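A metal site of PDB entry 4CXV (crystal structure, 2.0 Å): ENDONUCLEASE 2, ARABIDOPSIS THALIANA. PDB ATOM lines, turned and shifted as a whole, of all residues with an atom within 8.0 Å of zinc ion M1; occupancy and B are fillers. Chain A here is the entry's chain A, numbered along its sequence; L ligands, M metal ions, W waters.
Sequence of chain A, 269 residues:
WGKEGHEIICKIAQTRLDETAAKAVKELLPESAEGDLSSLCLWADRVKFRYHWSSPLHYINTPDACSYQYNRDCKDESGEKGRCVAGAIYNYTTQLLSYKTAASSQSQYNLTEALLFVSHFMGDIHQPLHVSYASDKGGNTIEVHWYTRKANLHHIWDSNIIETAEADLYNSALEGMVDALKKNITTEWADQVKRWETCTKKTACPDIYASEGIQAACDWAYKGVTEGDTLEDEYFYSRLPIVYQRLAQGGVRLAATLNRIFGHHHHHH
OD1 of Asp 158 lies close to N of Trp 1, at 3.0 Å.
The side-chain carboxylate (OD1) of Asp 158 is in hydrogen-bond range of the side-chain amide nitrogen (NE2) of Gln 127.
The backbone carbonyl oxygen (O) of Asp 158 is in hydrogen-bond range of the backbone NH (N) of Gly 2, 3.0 Å away.
A ring nitrogen (ND1) of His 130 lies within hydrogen-bond range of the backbone carbonyl oxygen (O) of His 58 (2.6 Å).
A ring nitrogen (ND1) of His 154 is in hydrogen-bond range of the backbone carbonyl oxygen (O) of Gly 138, at 2.7 Å.
The backbone NH (N) of His 154 lies within hydrogen-bond range of the side-chain amide oxygen (OD1) of Asn 152 (3.2 Å).
Within 4 Å of zinc ion M1: His 130, His 154 and Asp 158.
The nearest printed residue that does not touch zinc ion M1 is Trp 1 (4.2 Å).
Zinc ion M1 is bound by water W1.
Zinc ion M1 is bound by OD2 of Asp 158, 2.1 Å away.
Zinc ion M1 is bound by an oxygen (O4) of the ligand.
A ring nitrogen (NE2) of His 130 is bound to zinc ion M1, at 2.1 Å.
NE2 of His 154 binds zinc ion M1 (2.3 Å).
Slightly farther from zinc ion M1 lies OD1 of Asp 158 (2.6 Å).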
ATOM      1  N   TRP A   1      15.064  26.131 -26.353  1.00  0.00           N
ATOM      2  CA  TRP A   1      14.244  26.383 -25.156  1.00  0.00           C
ATOM      3  C   TRP A   1      14.176  25.177 -24.257  1.00  0.00           C
ATOM      4  O   TRP A   1      14.305  24.053 -24.705  1.00  0.00           O
ATOM      5  CB  TRP A   1      12.788  26.757 -25.502  1.00  0.00           C
ATOM      6  CG  TRP A   1      12.661  27.772 -26.564  1.00  0.00           C
ATOM      7  CD1 TRP A   1      12.393  27.542 -27.865  1.00  0.00           C
ATOM      8  CD2 TRP A   1      12.731  29.203 -26.407  1.00  0.00           C
ATOM      9  NE1 TRP A   1      12.324  28.742 -28.549  1.00  0.00           N
ATOM     10  CE2 TRP A   1      12.544  29.768 -27.669  1.00  0.00           C
ATOM     11  CE3 TRP A   1      12.953  30.042 -25.303  1.00  0.00           C
ATOM     12  CZ2 TRP A   1      12.584  31.147 -27.880  1.00  0.00           C
ATOM     13  CZ3 TRP A   1      12.984  31.404 -25.519  1.00  0.00           C
ATOM     14  CH2 TRP A   1      12.813  31.943 -26.803  1.00  0.00           C
ATOM     15  N   GLY A   2      13.911  25.443 -22.990  1.00  0.00           N
ATOM     16  CA  GLY A   2      13.498  24.386 -22.054  1.00  0.00           C
ATOM     17  C   GLY A   2      12.036  24.013 -22.243  1.00  0.00           C
ATOM     18  O   GLY A   2      11.379  24.378 -23.204  1.00  0.00           O
ATOM     19  N   HIS A   6       9.027  25.321 -25.268  1.00  0.00           N
ATOM     20  CA  HIS A   6       8.501  24.400 -26.283  1.00  0.00           C
ATOM     21  C   HIS A   6       6.999  24.149 -26.100  1.00  0.00           C
ATOM     22  O   HIS A   6       6.265  24.049 -27.081  1.00  0.00           O
ATOM     23  CB  HIS A   6       9.300  23.077 -26.305  1.00  0.00           C
ATOM     24  CG  HIS A   6      10.675  23.207 -26.885  1.00  0.00           C
ATOM     25  ND1 HIS A   6      10.895  23.334 -28.231  1.00  0.00           N
ATOM     26  CD2 HIS A   6      11.892  23.247 -26.298  1.00  0.00           C
ATOM     27  CE1 HIS A   6      12.192  23.415 -28.460  1.00  0.00           C
ATOM     28  NE2 HIS A   6      12.813  23.413 -27.301  1.00  0.00           N
ATOM     29  N   ASP A  45      14.692  16.560 -27.269  1.00  0.00           N
ATOM     30  CA  ASP A  45      15.789  16.776 -26.310  1.00  0.00           C
ATOM     31  C   ASP A  45      16.217  15.455 -25.623  1.00  0.00           C
ATOM     32  O   ASP A  45      17.370  15.300 -25.276  1.00  0.00           O
ATOM     33  CB  ASP A  45      15.414  17.812 -25.238  1.00  0.00           C
ATOM     34  CG  ASP A  45      15.758  19.259 -25.660  1.00  0.00           C
ATOM     35  OD1 ASP A  45      16.312  19.494 -26.759  1.00  0.00           O
ATOM     36  OD2 ASP A  45      15.447  20.160 -24.872  1.00  0.00           O
ATOM     37  N   LYS A  48      18.959  13.228 -27.652  1.00  0.00           N
ATOM     38  CA  LYS A  48      20.282  13.776 -27.948  1.00  0.00           C
ATOM     39  C   LYS A  48      21.421  12.755 -27.901  1.00  0.00           C
ATOM     40  O   LYS A  48      22.419  12.960 -28.583  1.00  0.00           O
ATOM     41  CB  LYS A  48      20.584  14.957 -27.028  1.00  0.00           C
ATOM     42  CG  LYS A  48      19.815  16.207 -27.369  1.00  0.00           C
ATOM     43  CD  LYS A  48      20.326  17.398 -26.557  1.00  0.00           C
ATOM     44  CE  LYS A  48      19.535  18.634 -26.846  1.00  0.00           C
ATOM     45  NZ  LYS A  48      19.776  19.705 -25.825  1.00  0.00           N
ATOM     46  N   HIS A  58      20.022  20.862 -32.957  1.00  0.00           N
ATOM     47  CA  HIS A  58      19.253  21.769 -32.108  1.00  0.00           C
ATOM     48  C   HIS A  58      19.690  23.229 -32.231  1.00  0.00           C
ATOM     49  O   HIS A  58      18.981  24.112 -31.723  1.00  0.00           O
ATOM     50  CB  HIS A  58      19.329  21.314 -30.638  1.00  0.00           C
ATOM     51  CG  HIS A  58      18.672  19.984 -30.389  1.00  0.00           C
ATOM     52  ND1 HIS A  58      17.528  19.860 -29.633  1.00  0.00           N
ATOM     53  CD2 HIS A  58      18.976  18.732 -30.794  1.00  0.00           C
ATOM     54  CE1 HIS A  58      17.164  18.587 -29.576  1.00  0.00           C
ATOM     55  NE2 HIS A  58      18.027  17.881 -30.273  1.00  0.00           N
ATOM     56  N   TYR A  59      20.803  23.516 -32.881  1.00  0.00           N
ATOM     57  CA  TYR A  59      21.347  24.868 -32.846  1.00  0.00           C
ATOM     58  C   TYR A  59      22.177  25.148 -34.105  1.00  0.00           C
ATOM     59  O   TYR A  59      22.307  24.300 -34.994  1.00  0.00           O
ATOM     60  CB  TYR A  59      22.213  25.034 -31.585  1.00  0.00           C
ATOM     61  CG  TYR A  59      23.328  24.019 -31.511  1.00  0.00           C
ATOM     62  CD1 TYR A  59      24.503  24.209 -32.228  1.00  0.00           C
ATOM     63  CD2 TYR A  59      23.169  22.808 -30.813  1.00  0.00           C
ATOM     64  CE1 TYR A  59      25.521  23.270 -32.207  1.00  0.00           C
ATOM     65  CE2 TYR A  59      24.188  21.872 -30.759  1.00  0.00           C
ATOM     66  CZ  TYR A  59      25.359  22.117 -31.456  1.00  0.00           C
ATOM     67  OH  TYR A  59      26.350  21.208 -31.453  1.00  0.00           O
ATOM     68  N   HIS A 120       9.864  20.546 -32.390  1.00  0.00           N
ATOM     69  CA  HIS A 120      10.878  20.988 -31.466  1.00  0.00           C
ATOM     70  C   HIS A 120      11.878  21.953 -32.128  1.00  0.00           C
ATOM     71  O   HIS A 120      12.216  22.985 -31.557  1.00  0.00           O
ATOM     72  CB  HIS A 120      11.613  19.779 -30.901  1.00  0.00           C
ATOM     73  CG  HIS A 120      12.673  20.147 -29.914  1.00  0.00           C
ATOM     74  ND1 HIS A 120      12.418  20.247 -28.568  1.00  0.00           N
ATOM     75  CD2 HIS A 120      13.975  20.415 -30.068  1.00  0.00           C
ATOM     76  CE1 HIS A 120      13.536  20.548 -27.937  1.00  0.00           C
ATOM     77  NE2 HIS A 120      14.494  20.689 -28.827  1.00  0.00           N
ATOM     78  N   ASP A 124      13.384  25.623 -31.361  1.00  0.00           N
ATOM     79  CA  ASP A 124      14.766  25.940 -31.060  1.00  0.00           C
ATOM     80  C   ASP A 124      15.332  27.008 -31.997  1.00  0.00           C
ATOM     81  O   ASP A 124      16.125  27.819 -31.550  1.00  0.00           O
ATOM     82  CB  ASP A 124      15.658  24.735 -31.100  1.00  0.00           C
ATOM     83  CG  ASP A 124      15.711  24.023 -29.802  1.00  0.00           C
ATOM     84  OD1 ASP A 124      15.056  24.439 -28.813  1.00  0.00           O
ATOM     85  OD2 ASP A 124      16.388  23.030 -29.774  1.00  0.00           O
ATOM     86  N   GLN A 127      14.992  30.413 -30.509  1.00  0.00           N
ATOM     87  CA  GLN A 127      15.682  30.798 -29.280  1.00  0.00           C
ATOM     88  C   GLN A 127      16.973  31.538 -29.760  1.00  0.00           C
ATOM     89  O   GLN A 127      17.798  30.958 -30.461  1.00  0.00           O
ATOM     90  CB  GLN A 127      16.060  29.551 -28.462  1.00  0.00           C
ATOM     91  CG  GLN A 127      16.135  29.759 -26.953  1.00  0.00           C
ATOM     92  CD  GLN A 127      17.389  30.459 -26.485  1.00  0.00           C
ATOM     93  OE1 GLN A 127      17.694  31.593 -26.914  1.00  0.00           O
ATOM     94  NE2 GLN A 127      18.089  29.846 -25.543  1.00  0.00           N
ATOM     95  N   LEU A 129      19.832  32.379 -28.630  1.00  0.00           N
ATOM     96  CA  LEU A 129      21.108  31.766 -28.336  1.00  0.00           C
ATOM     97  C   LEU A 129      21.281  30.356 -28.892  1.00  0.00           C
ATOM     98  O   LEU A 129      22.327  29.765 -28.701  1.00  0.00           O
ATOM     99  CB  LEU A 129      21.436  31.855 -26.837  1.00  0.00           C
ATOM    100  CG  LEU A 129      21.696  33.280 -26.372  1.00  0.00           C
ATOM    101  CD1 LEU A 129      22.046  33.325 -24.882  1.00  0.00           C
ATOM    102  CD2 LEU A 129      22.809  33.929 -27.164  1.00  0.00           C
ATOM    103  N   HIS A 130      20.288  29.856 -29.636  1.00  0.00           N
ATOM    104  CA  HIS A 130      20.495  28.690 -30.489  1.00  0.00           C
ATOM    105  C   HIS A 130      21.025  29.059 -31.879  1.00  0.00           C
ATOM    106  O   HIS A 130      21.211  28.171 -32.685  1.00  0.00           O
ATOM    107  CB  HIS A 130      19.194  27.858 -30.576  1.00  0.00           C
ATOM    108  CG  HIS A 130      18.994  26.954 -29.409  1.00  0.00           C
ATOM    109  ND1 HIS A 130      18.950  25.580 -29.528  1.00  0.00           N
ATOM    110  CD2 HIS A 130      18.861  27.214 -28.081  1.00  0.00           C
ATOM    111  CE1 HIS A 130      18.790  25.033 -28.339  1.00  0.00           C
ATOM    112  NE2 HIS A 130      18.715  26.000 -27.440  1.00  0.00           N
ATOM    113  N   LYS A 137      29.877  28.841 -26.941  1.00  0.00           N
ATOM    114  CA  LYS A 137      28.937  27.739 -26.993  1.00  0.00           C
ATOM    115  C   LYS A 137      27.507  28.251 -26.855  1.00  0.00           C
ATOM    116  O   LYS A 137      26.720  27.769 -26.028  1.00  0.00           O
ATOM    117  CB  LYS A 137      29.224  26.696 -25.926  1.00  0.00           C
ATOM    118  CG  LYS A 137      30.605  26.073 -26.030  1.00  0.00           C
ATOM    119  CD  LYS A 137      30.609  24.689 -25.399  1.00  0.00           C
ATOM    120  N   GLY A 138      27.167  29.249 -27.638  1.00  0.00           N
ATOM    121  CA  GLY A 138      25.829  29.807 -27.597  1.00  0.00           C
ATOM    122  C   GLY A 138      25.463  30.410 -26.259  1.00  0.00           C
ATOM    123  O   GLY A 138      24.312  30.325 -25.821  1.00  0.00           O
ATOM    124  N   ASN A 140      26.521  29.306 -23.394  1.00  0.00           N
ATOM    125  CA  ASN A 140      26.655  28.311 -22.338  1.00  0.00           C
ATOM    126  C   ASN A 140      27.854  28.527 -21.450  1.00  0.00           C
ATOM    127  O   ASN A 140      27.821  28.121 -20.309  1.00  0.00           O
ATOM    128  CB  ASN A 140      26.738  26.901 -22.889  1.00  0.00           C
ATOM    129  CG  ASN A 140      25.401  26.267 -23.041  1.00  0.00           C
ATOM    130  OD1 ASN A 140      24.796  25.845 -22.053  1.00  0.00           O
ATOM    131  ND2 ASN A 140      24.917  26.171 -24.279  1.00  0.00           N
ATOM    132  N   ASN A 152      24.128  30.108 -16.438  1.00  0.00           N
ATOM    133  CA  ASN A 152      24.771  30.605 -17.653  1.00  0.00           C
ATOM    134  C   ASN A 152      23.744  31.278 -18.560  1.00  0.00           C
ATOM    135  O   ASN A 152      22.520  31.082 -18.438  1.00  0.00           O
ATOM    136  CB  ASN A 152      25.511  29.494 -18.418  1.00  0.00           C
ATOM    137  CG  ASN A 152      24.597  28.401 -18.921  1.00  0.00           C
ATOM    138  OD1 ASN A 152      23.876  28.584 -19.902  1.00  0.00           O
ATOM    139  ND2 ASN A 152      24.655  27.245 -18.295  1.00  0.00           N
ATOM    140  N   HIS A 154      22.964  31.075 -21.695  1.00  0.00           N
ATOM    141  CA  HIS A 154      22.148  30.211 -22.522  1.00  0.00           C
ATOM    142  C   HIS A 154      20.913  29.709 -21.776  1.00  0.00           C
ATOM    143  O   HIS A 154      19.788  29.762 -22.281  1.00  0.00           O
ATOM    144  CB  HIS A 154      22.941  29.051 -23.024  1.00  0.00           C
ATOM    145  CG  HIS A 154      22.219  28.258 -24.046  1.00  0.00           C
ATOM    146  ND1 HIS A 154      22.352  28.479 -25.398  1.00  0.00           N
ATOM    147  CD2 HIS A 154      21.267  27.298 -23.906  1.00  0.00           C
ATOM    148  CE1 HIS A 154      21.564  27.649 -26.046  1.00  0.00           C
ATOM    149  NE2 HIS A 154      20.894  26.927 -25.163  1.00  0.00           N
ATOM    150  N   HIS A 155      21.148  29.215 -20.572  1.00  0.00           N
ATOM    151  CA  HIS A 155      20.076  28.686 -19.745  1.00  0.00           C
ATOM    152  C   HIS A 155      19.056  29.771 -19.381  1.00  0.00           C
ATOM    153  O   HIS A 155      17.859  29.518 -19.273  1.00  0.00           O
ATOM    154  CB  HIS A 155      20.672  28.053 -18.470  1.00  0.00           C
ATOM    155  CG  HIS A 155      19.701  27.193 -17.690  1.00  0.00           C
ATOM    156  ND1 HIS A 155      18.840  27.718 -16.745  1.00  0.00           N
ATOM    157  CD2 HIS A 155      19.484  25.857 -17.691  1.00  0.00           C
ATOM    158  CE1 HIS A 155      18.115  26.744 -16.209  1.00  0.00           C
ATOM    159  NE2 HIS A 155      18.485  25.602 -16.770  1.00  0.00           N
ATOM    160  N   TRP A 157      18.128  32.188 -21.261  1.00  0.00           N
ATOM    161  CA  TRP A 157      17.269  32.307 -22.434  1.00  0.00           C
ATOM    162  C   TRP A 157      16.422  31.064 -22.669  1.00  0.00           C
ATOM    163  O   TRP A 157      15.265  31.177 -23.073  1.00  0.00           O
ATOM    164  CB  TRP A 157      18.090  32.707 -23.639  1.00  0.00           C
ATOM    165  CG  TRP A 157      18.406  34.180 -23.521  1.00  0.00           C
ATOM    166  CD1 TRP A 157      19.307  34.780 -22.705  1.00  0.00           C
ATOM    167  CD2 TRP A 157      17.685  35.236 -24.153  1.00  0.00           C
ATOM    168  NE1 TRP A 157      19.271  36.152 -22.862  1.00  0.00           N
ATOM    169  CE2 TRP A 157      18.257  36.451 -23.741  1.00  0.00           C
ATOM    170  CE3 TRP A 157      16.626  35.256 -25.069  1.00  0.00           C
ATOM    171  CZ2 TRP A 157      17.798  37.665 -24.170  1.00  0.00           C
ATOM    172  CZ3 TRP A 157      16.168  36.463 -25.522  1.00  0.00           C
ATOM    173  CH2 TRP A 157      16.768  37.669 -25.085  1.00  0.00           C
ATOM    174  N   ASP A 158      16.948  29.873 -22.415  1.00  0.00           N
ATOM    175  CA  ASP A 158      16.127  28.675 -22.564  1.00  0.00           C
ATOM    176  C   ASP A 158      14.968  28.647 -21.568  1.00  0.00           C
ATOM    177  O   ASP A 158      13.836  28.291 -21.958  1.00  0.00           O
ATOM    178  CB  ASP A 158      16.941  27.406 -22.334  1.00  0.00           C
ATOM    179  CG  ASP A 158      17.614  26.905 -23.571  1.00  0.00           C
ATOM    180  OD1 ASP A 158      17.300  27.339 -24.696  1.00  0.00           O
ATOM    181  OD2 ASP A 158      18.497  26.028 -23.420  1.00  0.00           O
ATOM    182  N   SER A 159      15.262  29.050 -20.317  1.00  0.00           N
ATOM    183  CA  SER A 159      14.317  28.816 -19.227  1.00  0.00           C
ATOM    184  C   SER A 159      14.068  29.949 -18.249  1.00  0.00           C
ATOM    185  O   SER A 159      12.934  30.245 -17.928  1.00  0.00           O
ATOM    186  CB  SER A 159      14.731  27.589 -18.429  1.00  0.00           C
ATOM    187  OG  SER A 159      14.682  26.449 -19.260  1.00  0.00           O
HETATM  188  P1  LIG L   1      17.261  22.629 -26.060  1.00  0.00           P
HETATM  189  O1  LIG L   1      17.096  21.857 -24.756  1.00  0.00           O
HETATM  190  O2  LIG L   1      15.945  22.767 -26.772  1.00  0.00           O
HETATM  191  O3  LIG L   1      18.047  21.919 -27.122  1.00  0.00           O
HETATM  192  O4  LIG L   1      17.705  23.963 -25.573  1.00  0.00           O
HETATM  193 ZN    ZN M   1      19.095  25.555 -25.375  1.00  0.00          ZN
HETATM  194 ZN    ZN M   2      14.657  24.016 -26.852  1.00  0.00          ZN
HETATM  195 ZN    ZN M   3      16.465  21.382 -28.357  1.00  0.00          ZN
HETATM  196  O   HOH W   1      20.410  24.346 -25.232  1.00  0.00           O
